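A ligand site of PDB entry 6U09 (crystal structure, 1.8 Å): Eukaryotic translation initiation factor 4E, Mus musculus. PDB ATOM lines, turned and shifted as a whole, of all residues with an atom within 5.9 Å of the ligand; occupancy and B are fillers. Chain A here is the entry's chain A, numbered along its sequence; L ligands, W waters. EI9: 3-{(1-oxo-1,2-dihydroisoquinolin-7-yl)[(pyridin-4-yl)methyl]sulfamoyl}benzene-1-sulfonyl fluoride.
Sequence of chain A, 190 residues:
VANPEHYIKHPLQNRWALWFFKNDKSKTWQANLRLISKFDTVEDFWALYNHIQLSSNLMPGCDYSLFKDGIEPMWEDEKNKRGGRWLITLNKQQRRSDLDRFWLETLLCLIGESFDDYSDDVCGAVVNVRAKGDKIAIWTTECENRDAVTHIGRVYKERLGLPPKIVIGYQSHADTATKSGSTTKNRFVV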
ATOM      1  N   TRP A  19      12.218  20.656  -1.834  1.00  0.00           N
ATOM      2  CA  TRP A  19      11.949  22.095  -1.831  1.00  0.00           C
ATOM      3  C   TRP A  19      13.261  22.848  -2.003  1.00  0.00           C
ATOM      4  O   TRP A  19      14.314  22.372  -1.577  1.00  0.00           O
ATOM      5  CB  TRP A  19      11.321  22.523  -0.514  1.00  0.00           C
ATOM      6  CG  TRP A  19       9.945  21.968  -0.265  1.00  0.00           C
ATOM      7  CD1 TRP A  19       9.626  20.757   0.278  1.00  0.00           C
ATOM      8  CD2 TRP A  19       8.704  22.627  -0.540  1.00  0.00           C
ATOM      9  NE1 TRP A  19       8.253  20.628   0.365  1.00  0.00           N
ATOM     10  CE2 TRP A  19       7.670  21.767  -0.136  1.00  0.00           C
ATOM     11  CE3 TRP A  19       8.379  23.875  -1.072  1.00  0.00           C
ATOM     12  CZ2 TRP A  19       6.318  22.105  -0.261  1.00  0.00           C
ATOM     13  CZ3 TRP A  19       7.047  24.215  -1.196  1.00  0.00           C
ATOM     14  CH2 TRP A  19       6.037  23.329  -0.789  1.00  0.00           C
ATOM     15  N   PHE A  21      14.986  26.894  -1.642  1.00  0.00           N
ATOM     16  CA  PHE A  21      14.865  28.261  -1.155  1.00  0.00           C
ATOM     17  C   PHE A  21      16.068  29.040  -1.645  1.00  0.00           C
ATOM     18  O   PHE A  21      17.207  28.578  -1.547  1.00  0.00           O
ATOM     19  CB  PHE A  21      14.799  28.320   0.383  1.00  0.00           C
ATOM     20  CG  PHE A  21      14.689  29.733   0.918  1.00  0.00           C
ATOM     21  CD1 PHE A  21      13.467  30.276   1.212  1.00  0.00           C
ATOM     22  CD2 PHE A  21      15.816  30.519   1.095  1.00  0.00           C
ATOM     23  CE1 PHE A  21      13.377  31.577   1.694  1.00  0.00           C
ATOM     24  CE2 PHE A  21      15.719  31.798   1.578  1.00  0.00           C
ATOM     25  CZ  PHE A  21      14.489  32.331   1.871  1.00  0.00           C
ATOM     26  N   TRP A  29       9.604  35.566   2.823  1.00  0.00           N
ATOM     27  CA  TRP A  29      10.263  34.290   3.044  1.00  0.00           C
ATOM     28  C   TRP A  29       9.454  33.143   2.463  1.00  0.00           C
ATOM     29  O   TRP A  29      10.007  32.246   1.817  1.00  0.00           O
ATOM     30  CB  TRP A  29      10.511  34.029   4.536  1.00  0.00           C
ATOM     31  CG  TRP A  29      11.188  32.704   4.741  1.00  0.00           C
ATOM     32  CD1 TRP A  29      12.520  32.440   4.630  1.00  0.00           C
ATOM     33  CD2 TRP A  29      10.556  31.441   5.028  1.00  0.00           C
ATOM     34  NE1 TRP A  29      12.765  31.091   4.842  1.00  0.00           N
ATOM     35  CE2 TRP A  29      11.572  30.462   5.095  1.00  0.00           C
ATOM     36  CE3 TRP A  29       9.236  31.054   5.251  1.00  0.00           C
ATOM     37  CZ2 TRP A  29      11.316  29.124   5.377  1.00  0.00           C
ATOM     38  CZ3 TRP A  29       8.980  29.716   5.533  1.00  0.00           C
ATOM     39  CH2 TRP A  29      10.013  28.769   5.590  1.00  0.00           C
ATOM     40  N   LEU A  33      10.152  30.072  -0.925  1.00  0.00           N
ATOM     41  CA  LEU A  33      10.235  28.651  -0.680  1.00  0.00           C
ATOM     42  C   LEU A  33       9.448  27.923  -1.762  1.00  0.00           C
ATOM     43  O   LEU A  33       8.238  28.121  -1.872  1.00  0.00           O
ATOM     44  CB  LEU A  33       9.704  28.349   0.719  1.00  0.00           C
ATOM     45  CG  LEU A  33       9.535  26.948   1.260  1.00  0.00           C
ATOM     46  CD1 LEU A  33      10.866  26.202   1.223  1.00  0.00           C
ATOM     47  CD2 LEU A  33       8.990  27.070   2.676  1.00  0.00           C
ATOM     48  N   ASP A  63      18.760  27.004   0.326  1.00  0.00           N
ATOM     49  CA  ASP A  63      18.497  25.762   1.054  1.00  0.00           C
ATOM     50  C   ASP A  63      17.925  24.710   0.111  1.00  0.00           C
ATOM     51  O   ASP A  63      17.215  25.025  -0.829  1.00  0.00           O
ATOM     52  CB  ASP A  63      17.479  25.949   2.190  1.00  0.00           C
ATOM     53  CG  ASP A  63      17.751  27.213   3.025  1.00  0.00           C
ATOM     54  OD1 ASP A  63      18.911  27.449   3.412  1.00  0.00           O
ATOM     55  OD2 ASP A  63      16.775  27.945   3.304  1.00  0.00           O
ATOM     56  N   TYR A  64      18.227  23.434   0.382  1.00  0.00           N
ATOM     57  CA  TYR A  64      17.307  22.361  -0.030  1.00  0.00           C
ATOM     58  C   TYR A  64      16.546  21.832   1.186  1.00  0.00           C
ATOM     59  O   TYR A  64      17.062  21.802   2.301  1.00  0.00           O
ATOM     60  CB  TYR A  64      18.053  21.191  -0.651  1.00  0.00           C
ATOM     61  CG  TYR A  64      18.580  21.320  -2.051  1.00  0.00           C
ATOM     62  CD1 TYR A  64      19.940  21.114  -2.293  1.00  0.00           C
ATOM     63  CD2 TYR A  64      17.743  21.588  -3.135  1.00  0.00           C
ATOM     64  CE1 TYR A  64      20.463  21.158  -3.568  1.00  0.00           C
ATOM     65  CE2 TYR A  64      18.264  21.651  -4.422  1.00  0.00           C
ATOM     66  CZ  TYR A  64      19.631  21.449  -4.624  1.00  0.00           C
ATOM     67  OH  TYR A  64      20.197  21.471  -5.866  1.00  0.00           O
ATOM     68  N   SER A  65      15.327  21.333   0.960  1.00  0.00           N
ATOM     69  CA  SER A  65      14.752  20.561   2.048  1.00  0.00           C
ATOM     70  C   SER A  65      13.911  19.420   1.474  1.00  0.00           C
ATOM     71  O   SER A  65      13.400  19.491   0.348  1.00  0.00           O
ATOM     72  CB  SER A  65      13.951  21.440   3.021  1.00  0.00           C
ATOM     73  OG  SER A  65      12.838  22.038   2.406  1.00  0.00           O
ATOM     74  N   PHE A  67      10.813  16.969   2.630  1.00  0.00           N
ATOM     75  CA  PHE A  67       9.786  16.732   3.635  1.00  0.00           C
ATOM     76  C   PHE A  67       8.781  15.722   3.116  1.00  0.00           C
ATOM     77  O   PHE A  67       8.534  15.614   1.903  1.00  0.00           O
ATOM     78  CB  PHE A  67       9.062  18.034   4.010  1.00  0.00           C
ATOM     79  CG  PHE A  67       9.771  18.810   5.096  1.00  0.00           C
ATOM     80  CD1 PHE A  67      10.933  19.523   4.797  1.00  0.00           C
ATOM     81  CD2 PHE A  67       9.341  18.741   6.398  1.00  0.00           C
ATOM     82  CE1 PHE A  67      11.609  20.209   5.795  1.00  0.00           C
ATOM     83  CE2 PHE A  67      10.015  19.437   7.406  1.00  0.00           C
ATOM     84  CZ  PHE A  67      11.135  20.163   7.104  1.00  0.00           C
ATOM     85  N   PRO A  73       7.549  22.706   4.654  1.00  0.00           N
ATOM     86  CA  PRO A  73       8.875  22.918   5.232  1.00  0.00           C
ATOM     87  C   PRO A  73       8.953  24.193   6.066  1.00  0.00           C
ATOM     88  O   PRO A  73       9.761  25.098   5.797  1.00  0.00           O
ATOM     89  CB  PRO A  73       9.769  22.979   3.987  1.00  0.00           C
ATOM     90  CG  PRO A  73       8.907  23.529   2.947  1.00  0.00           C
ATOM     91  CD  PRO A  73       7.499  23.103   3.238  1.00  0.00           C
ATOM     92  N   MET A  74       8.116  24.291   7.106  1.00  0.00           N
ATOM     93  CA  MET A  74       8.225  25.412   7.999  1.00  0.00           C
ATOM     94  C   MET A  74       7.686  25.037   9.381  1.00  0.00           C
ATOM     95  O   MET A  74       6.818  24.176   9.513  1.00  0.00           O
ATOM     96  CB  MET A  74       7.514  26.672   7.454  1.00  0.00           C
ATOM     97  CG  MET A  74       6.128  26.451   6.874  1.00  0.00           C
ATOM     98  SD  MET A  74       5.660  27.783   5.718  1.00  0.00           S
ATOM     99  CE  MET A  74       5.791  29.240   6.756  1.00  0.00           C
ATOM    100  N   TRP A  75       8.242  25.706  10.393  1.00  0.00           N
ATOM    101  CA  TRP A  75       7.926  25.456  11.791  1.00  0.00           C
ATOM    102  C   TRP A  75       6.431  25.472  12.065  1.00  0.00           C
ATOM    103  O   TRP A  75       5.963  24.787  12.984  1.00  0.00           O
ATOM    104  CB  TRP A  75       8.550  26.513  12.697  1.00  0.00           C
ATOM    105  CG  TRP A  75      10.025  26.707  12.592  1.00  0.00           C
ATOM    106  CD1 TRP A  75      10.972  25.734  12.405  1.00  0.00           C
ATOM    107  CD2 TRP A  75      10.723  27.942  12.702  1.00  0.00           C
ATOM    108  NE1 TRP A  75      12.224  26.304  12.378  1.00  0.00           N
ATOM    109  CE2 TRP A  75      12.099  27.663  12.555  1.00  0.00           C
ATOM    110  CE3 TRP A  75      10.328  29.272  12.894  1.00  0.00           C
ATOM    111  CZ2 TRP A  75      13.080  28.653  12.603  1.00  0.00           C
ATOM    112  CZ3 TRP A  75      11.301  30.250  12.942  1.00  0.00           C
ATOM    113  CH2 TRP A  75      12.662  29.938  12.796  1.00  0.00           C
ATOM    114  N   GLU A  76       5.683  26.300  11.338  1.00  0.00           N
ATOM    115  CA  GLU A  76       4.278  26.523  11.627  1.00  0.00           C
ATOM    116  C   GLU A  76       3.380  25.389  11.160  1.00  0.00           C
ATOM    117  O   GLU A  76       2.201  25.357  11.545  1.00  0.00           O
ATOM    118  CB  GLU A  76       3.814  27.846  11.013  1.00  0.00           C
ATOM    119  CG  GLU A  76       4.542  29.069  11.557  1.00  0.00           C
ATOM    120  CD  GLU A  76       5.733  29.512  10.711  1.00  0.00           C
ATOM    121  OE1 GLU A  76       6.230  28.717   9.876  1.00  0.00           O
ATOM    122  OE2 GLU A  76       6.186  30.664  10.891  1.00  0.00           O
ATOM    123  N   ARG A  85      14.754  19.758  15.918  1.00  0.00           N
ATOM    124  CA  ARG A  85      15.683  19.240  14.914  1.00  0.00           C
ATOM    125  C   ARG A  85      17.004  18.805  15.533  1.00  0.00           C
ATOM    126  O   ARG A  85      17.482  19.408  16.494  1.00  0.00           O
ATOM    127  CB  ARG A  85      15.966  20.272  13.816  1.00  0.00           C
ATOM    128  CG  ARG A  85      16.761  21.464  14.335  1.00  0.00           C
ATOM    129  CD  ARG A  85      16.818  22.620  13.338  1.00  0.00           C
ATOM    130  NE  ARG A  85      17.647  23.725  13.843  1.00  0.00           N
ATOM    131  CZ  ARG A  85      17.997  24.788  13.118  1.00  0.00           C
ATOM    132  NH1 ARG A  85      18.759  25.733  13.647  1.00  0.00           N
ATOM    133  NH2 ARG A  85      17.579  24.896  11.855  1.00  0.00           N
ATOM    134  N   VAL A 126      16.764  19.481   6.179  1.00  0.00           N
ATOM    135  CA  VAL A 126      17.052  20.776   5.590  1.00  0.00           C
ATOM    136  C   VAL A 126      18.553  20.916   5.530  1.00  0.00           C
ATOM    137  O   VAL A 126      19.240  20.609   6.507  1.00  0.00           O
ATOM    138  CB  VAL A 126      16.457  21.951   6.420  1.00  0.00           C
ATOM    139  CG1 VAL A 126      16.874  23.274   5.807  1.00  0.00           C
ATOM    140  CG2 VAL A 126      14.917  21.850   6.547  1.00  0.00           C
ATOM    141  N   ASN A 128      21.219  24.067   4.806  1.00  0.00           N
ATOM    142  CA  ASN A 128      21.395  25.509   4.604  1.00  0.00           C
ATOM    143  C   ASN A 128      22.829  25.749   4.164  1.00  0.00           C
ATOM    144  O   ASN A 128      23.764  25.362   4.869  1.00  0.00           O
ATOM    145  CB  ASN A 128      21.130  26.294   5.884  1.00  0.00           C
ATOM    146  CG  ASN A 128      19.830  25.896   6.561  1.00  0.00           C
ATOM    147  OD1 ASN A 128      19.829  25.341   7.651  1.00  0.00           O
ATOM    148  ND2 ASN A 128      18.698  26.226   5.917  1.00  0.00           N
ATOM    149  N   ARG A 130      25.505  28.499   3.842  1.00  0.00           N
ATOM    150  CA  ARG A 130      25.688  29.853   4.367  1.00  0.00           C
ATOM    151  C   ARG A 130      27.161  30.199   4.445  1.00  0.00           C
ATOM    152  O   ARG A 130      28.002  29.352   4.786  1.00  0.00           O
ATOM    153  CB  ARG A 130      25.068  30.004   5.768  1.00  0.00           C
ATOM    154  CG  ARG A 130      23.556  29.803   5.840  1.00  0.00           C
ATOM    155  CD  ARG A 130      22.772  30.966   5.206  1.00  0.00           C
ATOM    156  NE  ARG A 130      21.321  30.782   5.422  1.00  0.00           N
ATOM    157  CZ  ARG A 130      20.577  29.903   4.761  1.00  0.00           C
ATOM    158  NH1 ARG A 130      21.124  29.141   3.827  1.00  0.00           N
ATOM    159  NH2 ARG A 130      19.276  29.784   5.012  1.00  0.00           N
ATOM    160  N   GLY A 133      29.009  29.251   7.607  1.00  0.00           N
ATOM    161  CA  GLY A 133      28.948  27.858   8.014  1.00  0.00           C
ATOM    162  C   GLY A 133      27.644  27.183   7.591  1.00  0.00           C
ATOM    163  O   GLY A 133      26.558  27.714   7.843  1.00  0.00           O
ATOM    164  N   LYS A 135      24.691  24.133   7.471  1.00  0.00           N
ATOM    165  CA  LYS A 135      23.985  23.377   8.480  1.00  0.00           C
ATOM    166  C   LYS A 135      23.150  22.310   7.773  1.00  0.00           C
ATOM    167  O   LYS A 135      22.623  22.543   6.688  1.00  0.00           O
ATOM    168  CB  LYS A 135      23.075  24.283   9.335  1.00  0.00           C
ATOM    169  CG  LYS A 135      23.806  25.331  10.158  1.00  0.00           C
ATOM    170  CD  LYS A 135      22.858  26.056  11.110  1.00  0.00           C
ATOM    171  CE  LYS A 135      22.585  27.467  10.654  1.00  0.00           C
ATOM    172  NZ  LYS A 135      21.438  27.526   9.732  1.00  0.00           N
ATOM    173  N   TRP A 139      14.400  17.137  10.952  1.00  0.00           N
ATOM    174  CA  TRP A 139      13.280  17.653  11.724  1.00  0.00           C
ATOM    175  C   TRP A 139      12.369  16.509  12.150  1.00  0.00           C
ATOM    176  O   TRP A 139      12.046  15.634  11.342  1.00  0.00           O
ATOM    177  CB  TRP A 139      12.473  18.638  10.877  1.00  0.00           C
ATOM    178  CG  TRP A 139      13.139  19.947  10.600  1.00  0.00           C
ATOM    179  CD1 TRP A 139      14.489  20.215  10.534  1.00  0.00           C
ATOM    180  CD2 TRP A 139      12.467  21.179  10.360  1.00  0.00           C
ATOM    181  NE1 TRP A 139      14.680  21.576  10.277  1.00  0.00           N
ATOM    182  CE2 TRP A 139      13.450  22.175  10.157  1.00  0.00           C
ATOM    183  CE3 TRP A 139      11.108  21.549  10.283  1.00  0.00           C
ATOM    184  CZ2 TRP A 139      13.131  23.499   9.882  1.00  0.00           C
ATOM    185  CZ3 TRP A 139      10.798  22.875  10.019  1.00  0.00           C
ATOM    186  CH2 TRP A 139      11.806  23.835   9.829  1.00  0.00           C
ATOM    187  N   THR A 176      14.253  27.706  18.735  1.00  0.00           N
ATOM    188  CA  THR A 176      14.980  28.233  17.577  1.00  0.00           C
ATOM    189  C   THR A 176      14.380  29.543  17.097  1.00  0.00           C
ATOM    190  O   THR A 176      15.102  30.493  16.770  1.00  0.00           O
ATOM    191  CB  THR A 176      14.993  27.188  16.466  1.00  0.00           C
ATOM    192  OG1 THR A 176      15.802  26.066  16.860  1.00  0.00           O
ATOM    193  CG2 THR A 176      15.546  27.772  15.166  1.00  0.00           C
HETATM  194  C1  EI9 L   1      10.362  28.485   9.375  1.00  0.00           C
HETATM  195  C10 EI9 L   1      14.572  26.370   4.357  1.00  0.00           C
HETATM  196  C11 EI9 L   1      13.761  25.461   3.694  1.00  0.00           C
HETATM  197  C12 EI9 L   1      12.825  24.760   5.710  1.00  0.00           C
HETATM  198  C13 EI9 L   1      13.615  25.650   6.434  1.00  0.00           C
HETATM  199  C14 EI9 L   1      16.946  27.993   9.620  1.00  0.00           C
HETATM  200  C15 EI9 L   1      16.527  28.898  10.583  1.00  0.00           C
HETATM  201  C16 EI9 L   1      17.415  29.793  11.162  1.00  0.00           C
HETATM  202  C17 EI9 L   1      18.750  29.798  10.778  1.00  0.00           C
HETATM  203  C18 EI9 L   1      19.209  28.899   9.816  1.00  0.00           C
HETATM  204  C19 EI9 L   1      18.301  28.001   9.236  1.00  0.00           C
HETATM  205  C2  EI9 L   1       9.607  30.695   9.432  1.00  0.00           C
HETATM  206  C20 EI9 L   1      12.725  28.044   8.621  1.00  0.00           C
HETATM  207  C21 EI9 L   1      11.693  28.949   8.887  1.00  0.00           C
HETATM  208  C3  EI9 L   1      10.832  31.185   8.977  1.00  0.00           C
HETATM  209  C4  EI9 L   1      11.879  30.313   8.710  1.00  0.00           C
HETATM  210  C5  EI9 L   1      13.105  30.794   8.256  1.00  0.00           C
HETATM  211  C6  EI9 L   1      14.137  29.889   7.989  1.00  0.00           C
HETATM  212  C7  EI9 L   1      13.962  28.516   8.167  1.00  0.00           C
HETATM  213  C8  EI9 L   1      15.403  27.458   6.478  1.00  0.00           C
HETATM  214  C9  EI9 L   1      14.496  26.471   5.752  1.00  0.00           C
HETATM  215  N1  EI9 L   1       9.392  29.387   9.615  1.00  0.00           N
HETATM  216  N2  EI9 L   1      15.039  27.658   7.881  1.00  0.00           N
HETATM  217  N3  EI9 L   1      12.912  24.696   4.374  1.00  0.00           N
HETATM  218  O1  EI9 L   1      10.143  27.268   9.563  1.00  0.00           O
HETATM  219  O2  EI9 L   1      15.016  26.503  10.023  1.00  0.00           O
HETATM  220  O3  EI9 L   1      16.575  25.842   8.411  1.00  0.00           O
HETATM  221  O4  EI9 L   1      21.466  29.951  10.095  1.00  0.00           O
HETATM  222  O5  EI9 L   1      20.865  29.141   7.974  1.00  0.00           O
HETATM  223  S1  EI9 L   1      15.880  26.965   8.967  1.00  0.00           S
HETATM  224  S2  EI9 L   1      20.755  28.933   9.382  1.00  0.00           S
HETATM  225  O   HOH W   1      16.935  23.327   9.870  1.00  0.00           O
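The backbone NH of Asn 128 is in hydrogen-bond range of the backbone carbonyl oxygen of Lys 135, 2.8 Å away. The guanidinium group (NH1) of Arg 130 lies within salt-bridge range of the side-chain carboxylate (OD1) of Asp 63, at 2.8 Å. The side-chain carboxylate (OD1) of Asp 63 lies within hydrogen-bond range of the side-chain amide nitrogen (ND2) of Asn 128 (2.8 Å). N of Asp 63 lies within hydrogen-bond range of O of Phe 21 (2.9 Å). The backbone carbonyl oxygen of Ser 65 lies within hydrogen-bond range of the backbone NH of Trp 19, 2.7 Å away.
O of Pro 73 lies close to N3 of the ligand (3.5 Å). NE1 of Trp 29 touches C5 of the ligand, at 3.4 Å. Leu 33 touches the ligand (CD1 to C11, 3.9 Å). Asp 63 touches the ligand. Met 74 touches the ligand (CA to O1, 3.1 Å). NH2 of Arg 85 touches O2 of the ligand, at 3.5 Å. Val 126 touches the ligand (CG1 to O3, 3.7 Å). Trp 139 touches the ligand. Within 4 Å of the ligand: Trp 29, Leu 33, Asp 63, Ser 65, Pro 73, Met 74, Trp 75, Glu 76, Arg 85, Val 126, Asn 128, Arg 130, Lys 135 and Trp 139.
A sulfur (S2) of the ligand is covalently linked to the side-chain amino group (NZ) of Lys 135 (1.6 Å). The backbone NH of Trp 75 lies within hydrogen-bond range of an oxygen (O1) of the ligand, 2.6 Å away. An oxygen (O5) of the ligand lies within hydrogen-bond range of the guanidinium group of Arg 130 (3.1 Å). A nitrogen (N1) of the ligand is in hydrogen-bond range of the side-chain carboxylate (OE1) of Glu 76 (3.2 Å). O3 of the ligand sits at hydrogen-bond distance from ND2 of Asn 128, at 3.3 Å. N3 of the ligand lies within hydrogen-bond range of OG of Ser 65, 3.3 Å away.
Water W1 lies within hydrogen-bond range of NH2 of Arg 85 (2.6 Å), NE1 of Trp 139 (2.9 Å) and O3 of the ligand (2.9 Å).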
